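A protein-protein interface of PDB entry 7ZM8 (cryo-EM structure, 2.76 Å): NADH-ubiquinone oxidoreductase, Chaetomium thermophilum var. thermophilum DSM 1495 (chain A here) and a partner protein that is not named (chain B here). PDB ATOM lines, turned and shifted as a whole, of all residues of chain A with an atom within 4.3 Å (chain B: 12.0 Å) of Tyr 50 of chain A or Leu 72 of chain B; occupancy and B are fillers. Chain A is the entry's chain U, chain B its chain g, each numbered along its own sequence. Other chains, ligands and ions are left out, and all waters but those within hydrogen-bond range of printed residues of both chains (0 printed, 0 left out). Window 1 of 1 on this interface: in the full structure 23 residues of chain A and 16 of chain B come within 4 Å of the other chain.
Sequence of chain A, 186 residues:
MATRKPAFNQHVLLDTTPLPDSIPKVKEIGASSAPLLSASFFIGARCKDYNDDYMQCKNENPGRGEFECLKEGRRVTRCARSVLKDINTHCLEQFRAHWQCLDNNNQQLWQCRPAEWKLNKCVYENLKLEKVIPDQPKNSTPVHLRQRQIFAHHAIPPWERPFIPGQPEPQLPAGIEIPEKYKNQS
Hydrophobic or aromatic side chains of chain A within 4 Å of the printed part of chain B: Tyr 50. Hydrophobic or aromatic side chains of chain B that line the printed part of chain A: Tyr 62, Pro 65, Leu 72 and Tyr 75. Among the printed residues, 11 pairs touch across the chains. Among the printed residues, Asp or Glu carboxylates within 4 Å of a Lys or Arg side-chain nitrogen of the other chain: Asp 49 of chain A with Lys 70 of chain B (3.2 Å) and Asp 53 of chain A with Arg 69 of chain B (3.0 Å).
CB of Asp 49 of chain A touches CD1 of Leu 72 of chain B (3.7 Å). CE1 of Tyr 50 of chain A touches CB of Leu 72 of chain B, at 3.7 Å. Gly 74 of chain B touches Tyr 50 of chain A (O to CE1, 3.9 Å). Tyr 75 of chain B touches Tyr 50 of chain A. CG of Asp 52 of chain A touches CG of Pro 65 of chain B (3.4 Å). Tyr 75 of chain B touches Cys 79 of chain A (CE2 to SG, 3.4 Å).
Of chain B, only Leu 72 (3.7 Å), Lys 73 (3.1 Å), Gly 74 (3.9 Å) and Tyr 75 (3.6 Å) come within 4 Å of Tyr 50 of chain A. No residue of chain B comes within 4 Å of Cys 47 of chain A. Asp 49 of chain A touches two residues of chain B. Asn 51 of chain A touches just one residue of chain B: Tyr 62 (3.4 Å). Asp 52 of chain A touches just these residues of chain B: Tyr 62 (2.7 Å) and Pro 65 (3.4 Å). No residue of chain B comes within 4 Å of Val 76 of chain A. Of the printed residues of chain A, Arg 69 of chain B touches Asp 53 (3.0 Å). Of the printed residues of chain A, Tyr 75 of chain B touches Tyr 50 (3.6 Å) and Cys 79 (3.4 Å). The nearest residue of chain B that does not touch Tyr 50 of chain A is Tyr 62 of chain B (6.5 Å). The nearest printed residue of chain A that does not touch Pro 65 of chain B is Asp 53 of chain A (5.7 Å).
The side-chain carboxylate (OD2) of Asp 49 of chain A lies within salt-bridge range of the side-chain amino group (NZ) of Lys 70 of chain B (3.2 Å). The side-chain hydroxyl (OH) of Tyr 50 of chain A lies within hydrogen-bond range of the backbone carbonyl oxygen (O) of Lys 73 of chain B (3.1 Å). The backbone carbonyl oxygen of Asn 51 of chain A is in hydrogen-bond range of the side-chain hydroxyl of Tyr 62 of chain B (3.4 Å). The side-chain hydroxyl (OH) of Tyr 62 of chain B lies within hydrogen-bond range of the side-chain carboxylate (OD1) of Asp 52 of chain A (2.7 Å). The guanidinium group of Arg 69 of chain B lies within salt-bridge range of the side-chain carboxylate of Asp 53 of chain A (3.0 Å).
The backbone carbonyl oxygen (O) of Cys 47 of chain A lies close to the side-chain amide oxygen (OD1) of Asn 51 of chain A (3.0 Å). SG of Cys 47 of chain A forms a disulfide with SG of Cys 79 of chain A, 2.0 Å away.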
ATOM      1  N   CYS A  47     -11.827  13.171 -17.093  1.00  0.00           N
ATOM      2  CA  CYS A  47     -13.149  12.616 -17.335  1.00  0.00           C
ATOM      3  C   CYS A  47     -13.569  11.614 -16.275  1.00  0.00           C
ATOM      4  O   CYS A  47     -14.614  10.977 -16.428  1.00  0.00           O
ATOM      5  CB  CYS A  47     -13.187  11.942 -18.704  1.00  0.00           C
ATOM      6  SG  CYS A  47     -12.972  13.066 -20.072  1.00  0.00           S
ATOM      7  N   LYS A  48     -12.787  11.465 -15.207  1.00  0.00           N
ATOM      8  CA  LYS A  48     -13.021  10.383 -14.258  1.00  0.00           C
ATOM      9  C   LYS A  48     -14.403  10.482 -13.632  1.00  0.00           C
ATOM     10  O   LYS A  48     -15.084   9.467 -13.454  1.00  0.00           O
ATOM     11  CB  LYS A  48     -11.940  10.395 -13.181  1.00  0.00           C
ATOM     12  CG  LYS A  48     -12.135   9.368 -12.078  1.00  0.00           C
ATOM     13  CD  LYS A  48     -10.976   9.398 -11.101  1.00  0.00           C
ATOM     14  CE  LYS A  48     -10.836  10.770 -10.463  1.00  0.00           C
ATOM     15  NZ  LYS A  48      -9.657  10.839  -9.556  1.00  0.00           N
ATOM     16  N   ASP A  49     -14.832  11.695 -13.283  1.00  0.00           N
ATOM     17  CA  ASP A  49     -16.145  11.868 -12.673  1.00  0.00           C
ATOM     18  C   ASP A  49     -17.255  11.457 -13.626  1.00  0.00           C
ATOM     19  O   ASP A  49     -18.229  10.815 -13.219  1.00  0.00           O
ATOM     20  CB  ASP A  49     -16.330  13.316 -12.229  1.00  0.00           C
ATOM     21  CG  ASP A  49     -15.398  13.698 -11.095  1.00  0.00           C
ATOM     22  OD1 ASP A  49     -14.180  13.821 -11.340  1.00  0.00           O
ATOM     23  OD2 ASP A  49     -15.882  13.873  -9.958  1.00  0.00           O
ATOM     24  N   TYR A  50     -17.119  11.823 -14.889  1.00  0.00           N
ATOM     25  CA  TYR A  50     -18.166  11.535 -15.894  1.00  0.00           C
ATOM     26  C   TYR A  50     -18.107  10.060 -16.244  1.00  0.00           C
ATOM     27  O   TYR A  50     -19.167   9.479 -16.434  1.00  0.00           O
ATOM     28  CB  TYR A  50     -17.932  12.426 -17.110  1.00  0.00           C
ATOM     29  CG  TYR A  50     -18.006  13.897 -16.801  1.00  0.00           C
ATOM     30  CD1 TYR A  50     -19.223  14.547 -16.742  1.00  0.00           C
ATOM     31  CD2 TYR A  50     -16.865  14.635 -16.548  1.00  0.00           C
ATOM     32  CE1 TYR A  50     -19.312  15.896 -16.455  1.00  0.00           C
ATOM     33  CE2 TYR A  50     -16.935  15.984 -16.250  1.00  0.00           C
ATOM     34  CZ  TYR A  50     -18.162  16.617 -16.203  1.00  0.00           C
ATOM     35  OH  TYR A  50     -18.244  17.947 -15.918  1.00  0.00           O
ATOM     36  N   ASN A  51     -16.908   9.485 -16.309  1.00  0.00           N
ATOM     37  CA  ASN A  51     -16.698   8.044 -16.621  1.00  0.00           C
ATOM     38  C   ASN A  51     -17.314   7.230 -15.497  1.00  0.00           C
ATOM     39  O   ASN A  51     -17.835   6.164 -15.773  1.00  0.00           O
ATOM     40  CB  ASN A  51     -15.232   7.709 -16.914  1.00  0.00           C
ATOM     41  CG  ASN A  51     -14.624   8.465 -18.066  1.00  0.00           C
ATOM     42  OD1 ASN A  51     -15.313   9.203 -18.758  1.00  0.00           O
ATOM     43  ND2 ASN A  51     -13.329   8.289 -18.267  1.00  0.00           N
ATOM     44  N   ASP A  52     -17.277   7.755 -14.286  1.00  0.00           N
ATOM     45  CA  ASP A  52     -17.777   7.009 -13.108  1.00  0.00           C
ATOM     46  C   ASP A  52     -19.282   7.188 -13.022  1.00  0.00           C
ATOM     47  O   ASP A  52     -19.948   6.206 -12.732  1.00  0.00           O
ATOM     48  CB  ASP A  52     -17.045   7.461 -11.850  1.00  0.00           C
ATOM     49  CG  ASP A  52     -15.650   6.889 -11.704  1.00  0.00           C
ATOM     50  OD1 ASP A  52     -15.401   5.801 -12.249  1.00  0.00           O
ATOM     51  OD2 ASP A  52     -14.825   7.538 -11.038  1.00  0.00           O
ATOM     52  N   ASP A  53     -19.788   8.366 -13.372  1.00  0.00           N
ATOM     53  CA  ASP A  53     -21.251   8.586 -13.372  1.00  0.00           C
ATOM     54  C   ASP A  53     -21.881   7.610 -14.358  1.00  0.00           C
ATOM     55  O   ASP A  53     -22.913   7.021 -14.019  1.00  0.00           O
ATOM     56  CB  ASP A  53     -21.592  10.025 -13.736  1.00  0.00           C
ATOM     57  CG  ASP A  53     -23.034  10.396 -13.457  1.00  0.00           C
ATOM     58  OD1 ASP A  53     -23.558   9.955 -12.420  1.00  0.00           O
ATOM     59  OD2 ASP A  53     -23.613  11.116 -14.282  1.00  0.00           O
ATOM     60  N   TYR A  54     -21.287   7.440 -15.526  1.00  0.00           N
ATOM     61  CA  TYR A  54     -21.907   6.591 -16.563  1.00  0.00           C
ATOM     62  C   TYR A  54     -22.005   5.149 -16.089  1.00  0.00           C
ATOM     63  O   TYR A  54     -23.057   4.532 -16.263  1.00  0.00           O
ATOM     64  CB  TYR A  54     -21.133   6.770 -17.862  1.00  0.00           C
ATOM     65  CG  TYR A  54     -21.459   5.804 -18.963  1.00  0.00           C
ATOM     66  CD1 TYR A  54     -22.626   5.922 -19.693  1.00  0.00           C
ATOM     67  CD2 TYR A  54     -20.581   4.786 -19.279  1.00  0.00           C
ATOM     68  CE1 TYR A  54     -22.916   5.041 -20.715  1.00  0.00           C
ATOM     69  CE2 TYR A  54     -20.854   3.894 -20.296  1.00  0.00           C
ATOM     70  CZ  TYR A  54     -22.025   4.027 -21.011  1.00  0.00           C
ATOM     71  OH  TYR A  54     -22.282   3.150 -22.011  1.00  0.00           O
ATOM     72  N   VAL A  76     -19.630  11.515 -21.567  1.00  0.00           N
ATOM     73  CA  VAL A  76     -18.278  10.893 -21.567  1.00  0.00           C
ATOM     74  C   VAL A  76     -17.578  11.088 -22.918  1.00  0.00           C
ATOM     75  O   VAL A  76     -16.377  11.327 -22.904  1.00  0.00           O
ATOM     76  CB  VAL A  76     -18.271   9.426 -21.091  1.00  0.00           C
ATOM     77  CG1 VAL A  76     -18.951   9.227 -19.755  1.00  0.00           C
ATOM     78  CG2 VAL A  76     -18.778   8.433 -22.118  1.00  0.00           C
ATOM     79  N   CYS A  79     -16.394  14.767 -23.180  1.00  0.00           N
ATOM     80  CA  CYS A  79     -15.295  15.091 -22.253  1.00  0.00           C
ATOM     81  C   CYS A  79     -14.025  14.445 -22.783  1.00  0.00           C
ATOM     82  O   CYS A  79     -12.961  15.065 -22.709  1.00  0.00           O
ATOM     83  CB  CYS A  79     -15.568  14.456 -20.899  1.00  0.00           C
ATOM     84  SG  CYS A  79     -14.206  14.660 -19.723  1.00  0.00           S
ATOM     85  N   TYR B  62     -14.216  -3.314 -13.811  1.00  0.00           N
ATOM     86  CA  TYR B  62     -14.222  -1.833 -13.712  1.00  0.00           C
ATOM     87  C   TYR B  62     -14.457  -1.454 -12.258  1.00  0.00           C
ATOM     88  O   TYR B  62     -15.382  -1.975 -11.624  1.00  0.00           O
ATOM     89  CB  TYR B  62     -15.300  -1.187 -14.583  1.00  0.00           C
ATOM     90  CG  TYR B  62     -15.274   0.318 -14.585  1.00  0.00           C
ATOM     91  CD1 TYR B  62     -15.871   1.044 -13.570  1.00  0.00           C
ATOM     92  CD2 TYR B  62     -14.639   1.016 -15.595  1.00  0.00           C
ATOM     93  CE1 TYR B  62     -15.835   2.427 -13.553  1.00  0.00           C
ATOM     94  CE2 TYR B  62     -14.600   2.397 -15.598  1.00  0.00           C
ATOM     95  CZ  TYR B  62     -15.196   3.104 -14.573  1.00  0.00           C
ATOM     96  OH  TYR B  62     -15.155   4.465 -14.586  1.00  0.00           O
ATOM     97  N   PRO B  63     -13.681  -0.494 -11.722  1.00  0.00           N
ATOM     98  CA  PRO B  63     -13.788  -0.148 -10.315  1.00  0.00           C
ATOM     99  C   PRO B  63     -14.938   0.824 -10.053  1.00  0.00           C
ATOM    100  O   PRO B  63     -14.703   2.012 -10.027  1.00  0.00           O
ATOM    101  CB  PRO B  63     -12.461   0.557 -10.077  1.00  0.00           C
ATOM    102  CG  PRO B  63     -12.125   1.208 -11.395  1.00  0.00           C
ATOM    103  CD  PRO B  63     -12.661   0.259 -12.435  1.00  0.00           C
ATOM    104  N   ILE B  64     -16.143   0.292  -9.834  1.00  0.00           N
ATOM    105  CA  ILE B  64     -17.339   1.151  -9.627  1.00  0.00           C
ATOM    106  C   ILE B  64     -17.097   1.954  -8.361  1.00  0.00           C
ATOM    107  O   ILE B  64     -16.613   1.377  -7.374  1.00  0.00           O
ATOM    108  CB  ILE B  64     -18.616   0.299  -9.535  1.00  0.00           C
ATOM    109  CG1 ILE B  64     -18.782  -0.609 -10.757  1.00  0.00           C
ATOM    110  CG2 ILE B  64     -19.852   1.158  -9.316  1.00  0.00           C
ATOM    111  CD1 ILE B  64     -19.384   0.078 -11.959  1.00  0.00           C
ATOM    112  N   PRO B  65     -17.460   3.250  -8.334  1.00  0.00           N
ATOM    113  CA  PRO B  65     -17.302   4.051  -7.138  1.00  0.00           C
ATOM    114  C   PRO B  65     -18.450   3.765  -6.152  1.00  0.00           C
ATOM    115  O   PRO B  65     -19.563   3.649  -6.629  1.00  0.00           O
ATOM    116  CB  PRO B  65     -17.521   5.474  -7.665  1.00  0.00           C
ATOM    117  CG  PRO B  65     -17.313   5.369  -9.145  1.00  0.00           C
ATOM    118  CD  PRO B  65     -17.902   4.025  -9.489  1.00  0.00           C
ATOM    119  N   PRO B  66     -18.239   3.637  -4.810  1.00  0.00           N
ATOM    120  CA  PRO B  66     -19.358   3.436  -3.889  1.00  0.00           C
ATOM    121  C   PRO B  66     -20.031   4.742  -3.500  1.00  0.00           C
ATOM    122  O   PRO B  66     -19.421   5.811  -3.480  1.00  0.00           O
ATOM    123  CB  PRO B  66     -18.680   2.788  -2.675  1.00  0.00           C
ATOM    124  CG  PRO B  66     -17.310   3.388  -2.669  1.00  0.00           C
ATOM    125  CD  PRO B  66     -16.953   3.737  -4.100  1.00  0.00           C
ATOM    126  N   GLY B  67     -21.318   4.633  -3.184  1.00  0.00           N
ATOM    127  CA  GLY B  67     -22.088   5.770  -2.740  1.00  0.00           C
ATOM    128  C   GLY B  67     -22.996   6.325  -3.818  1.00  0.00           C
ATOM    129  O   GLY B  67     -23.080   5.794  -4.929  1.00  0.00           O
ATOM    130  N   PRO B  68     -23.699   7.409  -3.504  1.00  0.00           N
ATOM    131  CA  PRO B  68     -24.606   8.014  -4.485  1.00  0.00           C
ATOM    132  C   PRO B  68     -23.843   8.680  -5.618  1.00  0.00           C
ATOM    133  O   PRO B  68     -22.659   9.005  -5.507  1.00  0.00           O
ATOM    134  CB  PRO B  68     -25.383   9.044  -3.660  1.00  0.00           C
ATOM    135  CG  PRO B  68     -24.454   9.399  -2.550  1.00  0.00           C
ATOM    136  CD  PRO B  68     -23.693   8.143  -2.228  1.00  0.00           C
ATOM    137  N   ARG B  69     -24.547   8.875  -6.730  1.00  0.00           N
ATOM    138  CA  ARG B  69     -23.953   9.533  -7.882  1.00  0.00           C
ATOM    139  C   ARG B  69     -23.721  11.009  -7.586  1.00  0.00           C
ATOM    140  O   ARG B  69     -24.362  11.599  -6.713  1.00  0.00           O
ATOM    141  CB  ARG B  69     -24.845   9.358  -9.110  1.00  0.00           C
ATOM    142  CG  ARG B  69     -24.985   7.905  -9.536  1.00  0.00           C
ATOM    143  CD  ARG B  69     -26.144   7.663 -10.480  1.00  0.00           C
ATOM    144  NE  ARG B  69     -25.844   8.071 -11.847  1.00  0.00           N
ATOM    145  CZ  ARG B  69     -26.545   8.968 -12.531  1.00  0.00           C
ATOM    146  NH1 ARG B  69     -26.200   9.275 -13.772  1.00  0.00           N
ATOM    147  NH2 ARG B  69     -27.597   9.553 -11.975  1.00  0.00           N
ATOM    148  N   LYS B  70     -22.784  11.606  -8.318  1.00  0.00           N
ATOM    149  CA  LYS B  70     -22.259  12.922  -7.981  1.00  0.00           C
ATOM    150  C   LYS B  70     -23.028  14.076  -8.604  1.00  0.00           C
ATOM    151  O   LYS B  70     -22.722  15.231  -8.294  1.00  0.00           O
ATOM    152  CB  LYS B  70     -20.785  13.024  -8.383  1.00  0.00           C
ATOM    153  CG  LYS B  70     -19.833  12.305  -7.446  1.00  0.00           C
ATOM    154  CD  LYS B  70     -18.391  12.589  -7.815  1.00  0.00           C
ATOM    155  CE  LYS B  70     -17.433  11.894  -6.865  1.00  0.00           C
ATOM    156  NZ  LYS B  70     -16.019  12.264  -7.145  1.00  0.00           N
ATOM    157  N   GLN B  71     -24.007  13.806  -9.469  1.00  0.00           N
ATOM    158  CA  GLN B  71     -24.832  14.854 -10.074  1.00  0.00           C
ATOM    159  C   GLN B  71     -23.954  15.871 -10.811  1.00  0.00           C
ATOM    160  O   GLN B  71     -23.820  17.035 -10.424  1.00  0.00           O
ATOM    161  CB  GLN B  71     -25.713  15.532  -9.017  1.00  0.00           C
ATOM    162  CG  GLN B  71     -26.755  16.484  -9.581  1.00  0.00           C
ATOM    163  CD  GLN B  71     -27.814  16.853  -8.564  1.00  0.00           C
ATOM    164  OE1 GLN B  71     -28.706  16.060  -8.263  1.00  0.00           O
ATOM    165  NE2 GLN B  71     -27.720  18.062  -8.025  1.00  0.00           N
ATOM    166  N   LEU B  72     -23.325  15.380 -11.872  1.00  0.00           N
ATOM    167  CA  LEU B  72     -22.365  16.177 -12.619  1.00  0.00           C
ATOM    168  C   LEU B  72     -23.058  17.287 -13.404  1.00  0.00           C
ATOM    169  O   LEU B  72     -24.252  17.219 -13.702  1.00  0.00           O
ATOM    170  CB  LEU B  72     -21.567  15.297 -13.579  1.00  0.00           C
ATOM    171  CG  LEU B  72     -20.353  14.522 -13.060  1.00  0.00           C
ATOM    172  CD1 LEU B  72     -19.278  15.486 -12.587  1.00  0.00           C
ATOM    173  CD2 LEU B  72     -20.725  13.534 -11.979  1.00  0.00           C
ATOM    174  N   LYS B  73     -22.288  18.321 -13.731  1.00  0.00           N
ATOM    175  CA  LYS B  73     -22.743  19.399 -14.598  1.00  0.00           C
ATOM    176  C   LYS B  73     -21.631  19.739 -15.577  1.00  0.00           C
ATOM    177  O   LYS B  73     -20.488  19.955 -15.166  1.00  0.00           O
ATOM    178  CB  LYS B  73     -23.139  20.642 -13.793  1.00  0.00           C
ATOM    179  CG  LYS B  73     -24.456  20.510 -13.050  1.00  0.00           C
ATOM    180  CD  LYS B  73     -25.601  20.230 -14.008  1.00  0.00           C
ATOM    181  CE  LYS B  73     -25.856  21.414 -14.925  1.00  0.00           C
ATOM    182  NZ  LYS B  73     -26.254  22.630 -14.164  1.00  0.00           N
ATOM    183  N   GLY B  74     -21.968  19.789 -16.862  1.00  0.00           N
ATOM    184  CA  GLY B  74     -20.988  20.066 -17.892  1.00  0.00           C
ATOM    185  C   GLY B  74     -21.010  19.032 -18.994  1.00  0.00           C
ATOM    186  O   GLY B  74     -21.580  17.954 -18.814  1.00  0.00           O
ATOM    187  N   TYR B  75     -20.398  19.352 -20.138  1.00  0.00           N
ATOM    188  CA  TYR B  75     -20.292  18.425 -21.265  1.00  0.00           C
ATOM    189  C   TYR B  75     -21.665  17.936 -21.720  1.00  0.00           C
ATOM    190  O   TYR B  75     -21.862  16.756 -22.011  1.00  0.00           O
ATOM    191  CB  TYR B  75     -19.382  17.249 -20.915  1.00  0.00           C
ATOM    192  CG  TYR B  75     -17.944  17.642 -20.732  1.00  0.00           C
ATOM    193  CD1 TYR B  75     -17.301  18.435 -21.665  1.00  0.00           C
ATOM    194  CD2 TYR B  75     -17.242  17.251 -19.609  1.00  0.00           C
ATOM    195  CE1 TYR B  75     -15.994  18.803 -21.500  1.00  0.00           C
ATOM    196  CE2 TYR B  75     -15.934  17.622 -19.429  1.00  0.00           C
ATOM    197  CZ  TYR B  75     -15.314  18.398 -20.380  1.00  0.00           C
ATOM    198  OH  TYR B  75     -14.002  18.771 -20.206  1.00  0.00           O
ATOM    199  N   ASP B  76     -22.624  18.848 -21.776  1.00  0.00           N
ATOM    200  CA  ASP B  76     -23.987  18.492 -22.120  1.00  0.00           C
ATOM    201  C   ASP B  76     -24.211  18.625 -23.623  1.00  0.00           C
ATOM    202  O   ASP B  76     -23.301  18.932 -24.394  1.00  0.00           O
ATOM    203  CB  ASP B  76     -24.973  19.353 -21.335  1.00  0.00           C
ATOM    204  CG  ASP B  76     -25.172  18.862 -19.918  1.00  0.00           C
ATOM    205  OD1 ASP B  76     -25.152  17.632 -19.706  1.00  0.00           O
ATOM    206  OD2 ASP B  76     -25.341  19.707 -19.015  1.00  0.00           O
ATOM    207  N   ASP B  77     -25.448  18.383 -24.043  1.00  0.00           N
ATOM    208  CA  ASP B  77     -25.775  18.425 -25.490  1.00  0.00           C
ATOM    209  C   ASP B  77     -25.459  19.805 -26.064  1.00  0.00           C
ATOM    210  O   ASP B  77     -25.051  19.871 -27.230  1.00  0.00           O
ATOM    211  CB  ASP B  77     -27.226  17.999 -25.714  1.00  0.00           C
ATOM    212  CG  ASP B  77     -27.522  16.596 -25.209  1.00  0.00           C
ATOM    213  OD1 ASP B  77     -26.815  15.661 -25.626  1.00  0.00           O
ATOM    214  OD2 ASP B  77     -28.453  16.453 -24.393  1.00  0.00           O
ATOM    215  N   ASP B  78     -25.626  20.864 -25.271  1.00  0.00           N
ATOM    216  CA  ASP B  78     -25.406  22.244 -25.781  1.00  0.00           C
ATOM    217  C   ASP B  78     -23.915  22.464 -26.064  1.00  0.00           C
ATOM    218  O   ASP B  78     -23.594  23.402 -26.817  1.00  0.00           O
ATOM    219  CB  ASP B  78     -25.979  23.298 -24.830  1.00  0.00           C
ATOM    220  CG  ASP B  78     -25.315  23.324 -23.464  1.00  0.00           C
ATOM    221  OD1 ASP B  78     -24.875  22.254 -23.003  1.00  0.00           O
ATOM    222  OD2 ASP B  78     -25.239  24.420 -22.874  1.00  0.00           O
ATOM    223  N   THR B  79     -23.043  21.634 -25.484  1.00  0.00           N
ATOM    224  CA  THR B  79     -21.577  21.801 -25.666  1.00  0.00           C
ATOM    225  C   THR B  79     -21.088  20.996 -26.874  1.00  0.00           C
ATOM    226  O   THR B  79     -19.879  21.073 -27.168  1.00  0.00           O
ATOM    227  CB  THR B  79     -20.804  21.394 -24.405  1.00  0.00           C
ATOM    228  OG1 THR B  79     -20.753  19.970 -24.349  1.00  0.00           O
ATOM    229  CG2 THR B  79     -21.410  21.949 -23.134  1.00  0.00           C
